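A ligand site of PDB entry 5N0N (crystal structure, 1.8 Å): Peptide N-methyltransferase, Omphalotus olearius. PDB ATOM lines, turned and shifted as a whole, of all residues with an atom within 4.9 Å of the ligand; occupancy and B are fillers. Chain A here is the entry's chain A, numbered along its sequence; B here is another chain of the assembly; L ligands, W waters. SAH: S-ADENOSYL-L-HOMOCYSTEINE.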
ATOM      1  N   ILE A  18       5.220   1.690  12.011  1.00  0.00           N
ATOM      2  CA  ILE A  18       4.782   1.525  13.409  1.00  0.00           C
ATOM      3  C   ILE A  18       5.549   2.430  14.382  1.00  0.00           C
ATOM      4  O   ILE A  18       4.936   3.122  15.192  1.00  0.00           O
ATOM      5  CB  ILE A  18       4.857   0.056  13.837  1.00  0.00           C
ATOM      6  CG1 ILE A  18       3.952  -0.808  12.950  1.00  0.00           C
ATOM      7  CG2 ILE A  18       4.500  -0.120  15.315  1.00  0.00           C
ATOM      8  CD1 ILE A  18       2.470  -0.483  13.012  1.00  0.00           C
ATOM      9  N   ILE A  43      -1.517   6.594  15.617  1.00  0.00           N
ATOM     10  CA  ILE A  43      -1.678   6.442  17.079  1.00  0.00           C
ATOM     11  C   ILE A  43      -0.849   7.448  17.873  1.00  0.00           C
ATOM     12  O   ILE A  43      -1.367   8.048  18.826  1.00  0.00           O
ATOM     13  CB  ILE A  43      -1.376   5.014  17.599  1.00  0.00           C
ATOM     14  CG1 ILE A  43      -2.295   3.984  16.924  1.00  0.00           C
ATOM     15  CG2 ILE A  43      -1.619   4.940  19.112  1.00  0.00           C
ATOM     16  CD1 ILE A  43      -1.910   2.542  17.219  1.00  0.00           C
ATOM     17  N   TYR A  97      -1.538   4.463   9.871  1.00  0.00           N
ATOM     18  CA  TYR A  97      -0.340   3.887  10.505  1.00  0.00           C
ATOM     19  C   TYR A  97      -0.041   2.470  10.022  1.00  0.00           C
ATOM     20  O   TYR A  97      -0.927   1.723   9.598  1.00  0.00           O
ATOM     21  CB  TYR A  97      -0.388   3.975  12.034  1.00  0.00           C
ATOM     22  CG  TYR A  97      -1.305   2.995  12.713  1.00  0.00           C
ATOM     23  CD1 TYR A  97      -2.665   3.241  12.837  1.00  0.00           C
ATOM     24  CD2 TYR A  97      -0.802   1.804  13.251  1.00  0.00           C
ATOM     25  CE1 TYR A  97      -3.501   2.330  13.475  1.00  0.00           C
ATOM     26  CE2 TYR A  97      -1.629   0.887  13.887  1.00  0.00           C
ATOM     27  CZ  TYR A  97      -2.982   1.162  13.990  1.00  0.00           C
ATOM     28  OH  TYR A  97      -3.842   0.273  14.627  1.00  0.00           O
ATOM     29  N   GLY A  98       1.239   2.110  10.081  1.00  0.00           N
ATOM     30  CA  GLY A  98       1.719   0.834   9.532  1.00  0.00           C
ATOM     31  C   GLY A  98       1.702   0.778   8.004  1.00  0.00           C
ATOM     32  O   GLY A  98       2.177   1.698   7.329  1.00  0.00           O
ATOM     33  N   HIS A  99       1.174  -0.322   7.479  1.00  0.00           N
ATOM     34  CA  HIS A  99       0.837  -0.492   6.050  1.00  0.00           C
ATOM     35  C   HIS A  99      -0.643  -0.140   5.904  1.00  0.00           C
ATOM     36  O   HIS A  99      -1.483  -0.720   6.609  1.00  0.00           O
ATOM     37  CB  HIS A  99       1.104  -1.953   5.647  1.00  0.00           C
ATOM     38  CG  HIS A  99       0.915  -2.276   4.194  1.00  0.00           C
ATOM     39  ND1 HIS A  99      -0.241  -1.982   3.496  1.00  0.00           N
ATOM     40  CD2 HIS A  99       1.699  -2.966   3.333  1.00  0.00           C
ATOM     41  CE1 HIS A  99      -0.140  -2.454   2.260  1.00  0.00           C
ATOM     42  NE2 HIS A  99       1.021  -3.061   2.138  1.00  0.00           N
ATOM     43  N   VAL A 102      -3.232  -3.209   5.349  1.00  0.00           N
ATOM     44  CA  VAL A 102      -3.103  -4.402   6.210  1.00  0.00           C
ATOM     45  C   VAL A 102      -3.992  -4.200   7.445  1.00  0.00           C
ATOM     46  O   VAL A 102      -3.687  -3.365   8.313  1.00  0.00           O
ATOM     47  CB  VAL A 102      -1.613  -4.616   6.593  1.00  0.00           C
ATOM     48  CG1 VAL A 102      -1.425  -5.651   7.698  1.00  0.00           C
ATOM     49  CG2 VAL A 102      -0.812  -5.032   5.358  1.00  0.00           C
ATOM     50  N   PHE A 103      -5.094  -4.958   7.515  1.00  0.00           N
ATOM     51  CA  PHE A 103      -6.108  -4.799   8.555  1.00  0.00           C
ATOM     52  C   PHE A 103      -6.670  -3.354   8.597  1.00  0.00           C
ATOM     53  O   PHE A 103      -6.763  -2.755   9.662  1.00  0.00           O
ATOM     54  CB  PHE A 103      -5.562  -5.262   9.939  1.00  0.00           C
ATOM     55  CG  PHE A 103      -5.259  -6.747  10.025  1.00  0.00           C
ATOM     56  CD1 PHE A 103      -4.139  -7.284   9.397  1.00  0.00           C
ATOM     57  CD2 PHE A 103      -6.092  -7.610  10.739  1.00  0.00           C
ATOM     58  CE1 PHE A 103      -3.851  -8.652   9.465  1.00  0.00           C
ATOM     59  CE2 PHE A 103      -5.819  -8.972  10.790  1.00  0.00           C
ATOM     60  CZ  PHE A 103      -4.705  -9.495  10.155  1.00  0.00           C
ATOM     61  N   VAL A 104      -7.027  -2.823   7.423  1.00  0.00           N
ATOM     62  CA  VAL A 104      -7.654  -1.485   7.267  1.00  0.00           C
ATOM     63  C   VAL A 104      -8.827  -1.543   6.256  1.00  0.00           C
ATOM     64  O   VAL A 104      -8.624  -1.901   5.112  1.00  0.00           O
ATOM     65  CB  VAL A 104      -6.643  -0.402   6.776  1.00  0.00           C
ATOM     66  CG1 VAL A 104      -7.294   0.979   6.725  1.00  0.00           C
ATOM     67  CG2 VAL A 104      -5.403  -0.354   7.651  1.00  0.00           C
ATOM     68  N   VAL A 127       5.477  -0.325   6.210  1.00  0.00           N
ATOM     69  CA  VAL A 127       5.938  -1.316   7.184  1.00  0.00           C
ATOM     70  C   VAL A 127       4.817  -1.680   8.157  1.00  0.00           C
ATOM     71  O   VAL A 127       4.366  -0.826   8.918  1.00  0.00           O
ATOM     72  CB  VAL A 127       7.157  -0.772   7.964  1.00  0.00           C
ATOM     73  CG1 VAL A 127       7.572  -1.718   9.081  1.00  0.00           C
ATOM     74  CG2 VAL A 127       8.314  -0.504   7.006  1.00  0.00           C
ATOM     75  N   SER A 128       4.386  -2.942   8.166  1.00  0.00           N
ATOM     76  CA  SER A 128       3.302  -3.387   9.059  1.00  0.00           C
ATOM     77  C   SER A 128       3.779  -3.862  10.431  1.00  0.00           C
ATOM     78  O   SER A 128       4.975  -4.089  10.661  1.00  0.00           O
ATOM     79  CB  SER A 128       2.533  -4.534   8.414  1.00  0.00           C
ATOM     80  OG  SER A 128       3.290  -5.742   8.477  1.00  0.00           O
ATOM     81  N   ALA A 129       2.829  -4.069  11.352  1.00  0.00           N
ATOM     82  CA  ALA A 129       3.134  -4.688  12.651  1.00  0.00           C
ATOM     83  C   ALA A 129       3.715  -6.104  12.511  1.00  0.00           C
ATOM     84  O   ALA A 129       4.540  -6.514  13.353  1.00  0.00           O
ATOM     85  CB  ALA A 129       1.904  -4.714  13.544  1.00  0.00           C
ATOM     86  N   GLU A 130       3.297  -6.841  11.475  1.00  0.00           N
ATOM     87  CA  GLU A 130       3.887  -8.162  11.183  1.00  0.00           C
ATOM     88  C   GLU A 130       5.346  -8.038  10.709  1.00  0.00           C
ATOM     89  O   GLU A 130       6.183  -8.847  11.090  1.00  0.00           O
ATOM     90  CB  GLU A 130       3.052  -8.937  10.155  1.00  0.00           C
ATOM     91  CG  GLU A 130       3.545 -10.371   9.958  1.00  0.00           C
ATOM     92  CD  GLU A 130       2.599 -11.261   9.196  1.00  0.00           C
ATOM     93  OE1 GLU A 130       2.618 -11.246   7.945  1.00  0.00           O
ATOM     94  OE2 GLU A 130       1.855 -12.027   9.848  1.00  0.00           O
ATOM     95  N   LEU A 169      -1.571 -13.800  15.082  1.00  0.00           N
ATOM     96  CA  LEU A 169      -2.961 -13.341  15.314  1.00  0.00           C
ATOM     97  C   LEU A 169      -3.007 -11.855  15.705  1.00  0.00           C
ATOM     98  O   LEU A 169      -2.471 -11.479  16.743  1.00  0.00           O
ATOM     99  CB  LEU A 169      -3.628 -14.187  16.419  1.00  0.00           C
ATOM    100  CG  LEU A 169      -3.763 -15.691  16.217  1.00  0.00           C
ATOM    101  CD1 LEU A 169      -4.387 -16.349  17.437  1.00  0.00           C
ATOM    102  CD2 LEU A 169      -4.601 -16.000  14.983  1.00  0.00           C
ATOM    103  N   PHE A 170      -3.658 -11.041  14.860  1.00  0.00           N
ATOM    104  CA  PHE A 170      -3.903  -9.601  15.119  1.00  0.00           C
ATOM    105  C   PHE A 170      -5.220  -9.423  15.928  1.00  0.00           C
ATOM    106  O   PHE A 170      -6.109 -10.274  15.864  1.00  0.00           O
ATOM    107  CB  PHE A 170      -4.075  -8.813  13.814  1.00  0.00           C
ATOM    108  CG  PHE A 170      -2.795  -8.454  13.076  1.00  0.00           C
ATOM    109  CD1 PHE A 170      -1.954  -9.437  12.553  1.00  0.00           C
ATOM    110  CD2 PHE A 170      -2.491  -7.115  12.817  1.00  0.00           C
ATOM    111  CE1 PHE A 170      -0.808  -9.076  11.835  1.00  0.00           C
ATOM    112  CE2 PHE A 170      -1.354  -6.749  12.101  1.00  0.00           C
ATOM    113  CZ  PHE A 170      -0.509  -7.731  11.620  1.00  0.00           C
ATOM    114  N   GLN A 171      -5.335  -8.293  16.629  1.00  0.00           N
ATOM    115  CA  GLN A 171      -6.575  -7.893  17.324  1.00  0.00           C
ATOM    116  C   GLN A 171      -7.030  -8.868  18.419  1.00  0.00           C
ATOM    117  O   GLN A 171      -8.227  -9.087  18.629  1.00  0.00           O
ATOM    118  CB  GLN A 171      -7.711  -7.567  16.319  1.00  0.00           C
ATOM    119  CG  GLN A 171      -7.261  -6.613  15.204  1.00  0.00           C
ATOM    120  CD  GLN A 171      -8.363  -5.807  14.536  1.00  0.00           C
ATOM    121  OE1 GLN A 171      -8.118  -4.703  14.048  1.00  0.00           O
ATOM    122  NE2 GLN A 171      -9.575  -6.351  14.507  1.00  0.00           N
ATOM    123  N   CSO A 174      -9.512  -7.346  21.297  1.00  0.00           N
ATOM    124  CA  CSO A 174     -10.941  -7.023  21.102  1.00  0.00           C
ATOM    125  CB  CSO A 174     -11.149  -5.730  20.304  1.00  0.00           C
ATOM    126  SG  CSO A 174     -10.171  -5.658  18.841  1.00  0.00           S
ATOM    127  C   CSO A 174     -11.703  -8.162  20.467  1.00  0.00           C
ATOM    128  O   CSO A 174     -12.374  -7.989  19.436  1.00  0.00           O
ATOM    129  OD  CSO A 174      -8.772  -4.940  19.569  1.00  0.00           O
ATOM    130  N   TYR A 210       3.336  -9.869  21.845  1.00  0.00           N
ATOM    131  CA  TYR A 210       4.200  -8.921  21.128  1.00  0.00           C
ATOM    132  C   TYR A 210       3.589  -7.519  21.024  1.00  0.00           C
ATOM    133  O   TYR A 210       2.459  -7.367  20.549  1.00  0.00           O
ATOM    134  CB  TYR A 210       4.519  -9.447  19.717  1.00  0.00           C
ATOM    135  CG  TYR A 210       5.363  -8.475  18.903  1.00  0.00           C
ATOM    136  CD1 TYR A 210       6.648  -8.128  19.314  1.00  0.00           C
ATOM    137  CD2 TYR A 210       4.871  -7.888  17.732  1.00  0.00           C
ATOM    138  CE1 TYR A 210       7.421  -7.236  18.589  1.00  0.00           C
ATOM    139  CE2 TYR A 210       5.641  -6.995  16.997  1.00  0.00           C
ATOM    140  CZ  TYR A 210       6.911  -6.672  17.432  1.00  0.00           C
ATOM    141  OH  TYR A 210       7.695  -5.786  16.713  1.00  0.00           O
ATOM    142  N   ILE A 211       4.346  -6.517  21.474  1.00  0.00           N
ATOM    143  CA  ILE A 211       4.024  -5.104  21.199  1.00  0.00           C
ATOM    144  C   ILE A 211       5.302  -4.410  20.706  1.00  0.00           C
ATOM    145  O   ILE A 211       6.272  -4.283  21.458  1.00  0.00           O
ATOM    146  CB  ILE A 211       3.470  -4.329  22.437  1.00  0.00           C
ATOM    147  CG1 ILE A 211       2.306  -5.089  23.091  1.00  0.00           C
ATOM    148  CG2 ILE A 211       3.019  -2.931  22.013  1.00  0.00           C
ATOM    149  CD1 ILE A 211       1.754  -4.437  24.351  1.00  0.00           C
ATOM    150  N   ALA A 212       5.282  -3.996  19.453  1.00  0.00           N
ATOM    151  CA  ALA A 212       6.378  -3.221  18.852  1.00  0.00           C
ATOM    152  C   ALA A 212       6.474  -1.850  19.528  1.00  0.00           C
ATOM    153  O   ALA A 212       5.432  -1.231  19.844  1.00  0.00           O
ATOM    154  CB  ALA A 212       6.148  -3.034  17.365  1.00  0.00           C
ATOM    155  N   MET A 214       6.660   1.953  19.855  1.00  0.00           N
ATOM    156  CA  MET A 214       6.130   3.059  19.057  1.00  0.00           C
ATOM    157  C   MET A 214       6.988   4.320  19.159  1.00  0.00           C
ATOM    158  O   MET A 214       6.920   5.155  18.265  1.00  0.00           O
ATOM    159  CB  MET A 214       4.663   3.312  19.445  1.00  0.00           C
ATOM    160  CG  MET A 214       3.767   2.184  18.955  1.00  0.00           C
ATOM    161  SD  MET A 214       2.072   2.176  19.561  1.00  0.00           S
ATOM    162  CE  MET A 214       1.578   3.743  18.889  1.00  0.00           C
ATOM    163  N   GLY A 241      -5.129  -2.935  22.892  1.00  0.00           N
ATOM    164  CA  GLY A 241      -5.443  -2.553  21.517  1.00  0.00           C
ATOM    165  C   GLY A 241      -4.311  -2.634  20.499  1.00  0.00           C
ATOM    166  O   GLY A 241      -4.583  -2.694  19.300  1.00  0.00           O
ATOM    167  N   VAL A 242      -3.060  -2.613  20.960  1.00  0.00           N
ATOM    168  CA  VAL A 242      -1.888  -2.770  20.072  1.00  0.00           C
ATOM    169  C   VAL A 242      -1.132  -4.098  20.315  1.00  0.00           C
ATOM    170  O   VAL A 242       0.044  -4.215  19.972  1.00  0.00           O
ATOM    171  CB  VAL A 242      -0.916  -1.557  20.136  1.00  0.00           C
ATOM    172  CG1 VAL A 242      -1.566  -0.332  19.529  1.00  0.00           C
ATOM    173  CG2 VAL A 242      -0.457  -1.269  21.568  1.00  0.00           C
ATOM    174  N   SER A 243      -1.823  -5.100  20.861  1.00  0.00           N
ATOM    175  CA  SER A 243      -1.236  -6.410  21.136  1.00  0.00           C
ATOM    176  C   SER A 243      -1.447  -7.382  19.958  1.00  0.00           C
ATOM    177  O   SER A 243      -2.536  -7.425  19.383  1.00  0.00           O
ATOM    178  CB  SER A 243      -1.852  -7.034  22.398  1.00  0.00           C
ATOM    179  OG  SER A 243      -1.561  -6.259  23.558  1.00  0.00           O
ATOM    180  N   THR A 244      -0.400  -8.149  19.640  1.00  0.00           N
ATOM    181  CA  THR A 244      -0.430  -9.220  18.631  1.00  0.00           C
ATOM    182  C   THR A 244       0.152 -10.497  19.287  1.00  0.00           C
ATOM    183  O   THR A 244       1.049 -10.395  20.111  1.00  0.00           O
ATOM    184  CB  THR A 244       0.401  -8.789  17.395  1.00  0.00           C
ATOM    185  OG1 THR A 244      -0.233  -7.675  16.765  1.00  0.00           O
ATOM    186  CG2 THR A 244       0.575  -9.907  16.363  1.00  0.00           C
ATOM    187  N   MVA B 400      -6.826   2.180  18.248  1.00  0.00           N
ATOM    188  CN  MVA B 400      -5.637   1.338  18.291  1.00  0.00           C
ATOM    189  CA  MVA B 400      -7.239   2.670  16.900  1.00  0.00           C
ATOM    190  CB  MVA B 400      -6.472   3.956  16.456  1.00  0.00           C
ATOM    191  CG1 MVA B 400      -5.286   3.788  15.521  1.00  0.00           C
ATOM    192  CG2 MVA B 400      -6.019   4.853  17.628  1.00  0.00           C
ATOM    193  C   MVA B 400      -7.332   1.519  15.894  1.00  0.00           C
ATOM    194  O   MVA B 400      -6.391   1.240  15.140  1.00  0.00           O
ATOM    195  N   ILE B 401      -8.468   0.818  15.915  1.00  0.00           N
ATOM    196  CA  ILE B 401      -8.658  -0.341  15.053  1.00  0.00           C
ATOM    197  C   ILE B 401      -9.424   0.060  13.774  1.00  0.00           C
ATOM    198  O   ILE B 401     -10.462   0.738  13.874  1.00  0.00           O
ATOM    199  CB  ILE B 401      -9.259  -1.563  15.787  1.00  0.00           C
ATOM    200  CG1 ILE B 401     -10.708  -1.324  16.252  1.00  0.00           C
ATOM    201  CG2 ILE B 401      -8.360  -1.960  16.964  1.00  0.00           C
ATOM    202  CD1 ILE B 401     -11.314  -2.523  16.968  1.00  0.00           C
ATOM    203  N   MVA B 402      -8.920  -0.305  12.591  1.00  0.00           N
ATOM    204  CN  MVA B 402      -7.837  -1.289  12.435  1.00  0.00           C
ATOM    205  CA  MVA B 402      -9.450   0.284  11.337  1.00  0.00           C
ATOM    206  CB  MVA B 402      -8.425   1.232  10.644  1.00  0.00           C
ATOM    207  CG1 MVA B 402      -7.365   1.876  11.564  1.00  0.00           C
ATOM    208  CG2 MVA B 402      -9.137   2.367   9.924  1.00  0.00           C
ATOM    209  C   MVA B 402     -10.039  -0.774  10.393  1.00  0.00           C
ATOM    210  O   MVA B 402     -10.041  -0.578   9.183  1.00  0.00           O
HETATM  211  N   SAH L   1      -2.344  -1.219   9.493  1.00  0.00           N
HETATM  212  CA  SAH L   1      -1.753  -1.747  10.764  1.00  0.00           C
HETATM  213  CB  SAH L   1      -2.722  -2.685  11.504  1.00  0.00           C
HETATM  214  CG  SAH L   1      -4.055  -2.050  11.909  1.00  0.00           C
HETATM  215  SD  SAH L   1      -5.158  -3.182  12.759  1.00  0.00           S
HETATM  216  C   SAH L   1      -0.471  -2.475  10.420  1.00  0.00           C
HETATM  217  O   SAH L   1       0.090  -3.237  11.233  1.00  0.00           O
HETATM  218  OXT SAH L   1       0.051  -2.339   9.319  1.00  0.00           O
HETATM  219  C5' SAH L   1      -4.732  -3.056  14.482  1.00  0.00           C
HETATM  220  C4' SAH L   1      -3.962  -4.280  14.990  1.00  0.00           C
HETATM  221  O4' SAH L   1      -2.613  -4.213  14.525  1.00  0.00           O
HETATM  222  C3' SAH L   1      -3.804  -4.418  16.503  1.00  0.00           C
HETATM  223  O3' SAH L   1      -4.921  -4.985  17.208  1.00  0.00           O
HETATM  224  C2' SAH L   1      -2.563  -5.292  16.611  1.00  0.00           C
HETATM  225  O2' SAH L   1      -2.870  -6.690  16.395  1.00  0.00           O
HETATM  226  C1' SAH L   1      -1.693  -4.761  15.475  1.00  0.00           C
HETATM  227  N9  SAH L   1      -0.769  -3.722  16.013  1.00  0.00           N
HETATM  228  C8  SAH L   1      -0.907  -2.374  15.930  1.00  0.00           C
HETATM  229  N7  SAH L   1       0.114  -1.735  16.535  1.00  0.00           N
HETATM  230  C5  SAH L   1       0.937  -2.674  17.037  1.00  0.00           C
HETATM  231  C6  SAH L   1       2.192  -2.696  17.819  1.00  0.00           C
HETATM  232  N6  SAH L   1       2.796  -1.523  18.180  1.00  0.00           N
HETATM  233  N1  SAH L   1       2.731  -3.900  18.136  1.00  0.00           N
HETATM  234  C2  SAH L   1       2.127  -5.072  17.775  1.00  0.00           C
HETATM  235  N3  SAH L   1       0.979  -5.129  17.081  1.00  0.00           N
HETATM  236  C4  SAH L   1       0.348  -3.986  16.693  1.00  0.00           C
HETATM  237  O   HOH W   1      -5.034  -6.366  19.972  1.00  0.00           O
HETATM  238  O   HOH W   2       1.364   0.769  16.995  1.00  0.00           O
HETATM  239  O   HOH W   3      -3.574   1.351  10.109  1.00  0.00           O
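O of Val 102 lies within hydrogen-bond range of N of the ligand, at 2.8 Å.
The side-chain hydroxyl (OG1) of Thr 244 is in hydrogen-bond range of a nitrogen (N3) of the ligand, 2.8 Å away.
O of the ligand lies within hydrogen-bond range of N of Ala 129 (2.9 Å).
N1 of the ligand is in hydrogen-bond range of N of Ala 212.
The backbone carbonyl oxygen of Ala 212 sits at hydrogen-bond distance from a nitrogen (N6) of the ligand (3.1 Å).
An oxygen (O2') of the ligand lies within hydrogen-bond range of the backbone NH (N) of Gln 171.
The side-chain amide oxygen of Gln 171 lies close to a sulfur (SD) of the ligand.
The backbone NH of His 99 sits at hydrogen-bond distance from an oxygen (OXT) of the ligand (3.0 Å).
O of His 99 is in hydrogen-bond range of N of the ligand, 3.1 Å away.
The backbone carbonyl oxygen of Ser 243 sits at hydrogen-bond distance from an oxygen (O2') of the ligand, at 3.1 Å.
O of Gly 241 is in hydrogen-bond range of O3' of the ligand, 3.1 Å away.
The backbone carbonyl oxygen of Tyr 97 sits at hydrogen-bond distance from a nitrogen (N) of the ligand (3.3 Å).
O of Thr 244 sits at hydrogen-bond distance from N of Tyr 210, 2.9 Å away.
The side-chain hydroxyl (OH) of Tyr 97 is in hydrogen-bond range of O of MVA 400 of chain B.
The side-chain hydroxyl (OG) of Ser 128 is in hydrogen-bond range of the backbone NH (N) of Glu 130 (3.2 Å).
A sulfur (SD) of the ligand lies close to the backbone carbonyl oxygen of Phe 103, at 3.5 Å.
O of Val 242 lies close to N3 of the ligand, 3.2 Å away.
CG2 of Ile 18 touches N6 of the ligand (3.6 Å).
CA of Gly 98 touches OXT of the ligand, 3.6 Å away.
CG2 of Val 104 touches N of the ligand (3.7 Å).
Ser 128 touches the ligand.
Phe 170 touches the ligand (CA to O2', 3.3 Å).
O of Tyr 210 touches C2 of the ligand (3.6 Å).
Ile 211 touches the ligand.
CG of Met 214 touches N6 of the ligand, 3.9 Å away.
MVA 402 of chain B touches the ligand (CN to SD, 3.3 Å).
Of the 27 residues printed, 20 come within 4 Å of the ligand.
The nearest printed residue that does not touch the ligand is CSO 174 (4.5 Å).
Water W2 bridges a nitrogen (N7) of the ligand (2.8 Å) and the side-chain sulfur (SD) of Met 214 (3.0 Å).
Water W3 bridges the backbone carbonyl oxygen of Tyr 97 and a nitrogen (N) of the ligand.
Water W1 bridges O of Ser 243 and O3' of the ligand.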
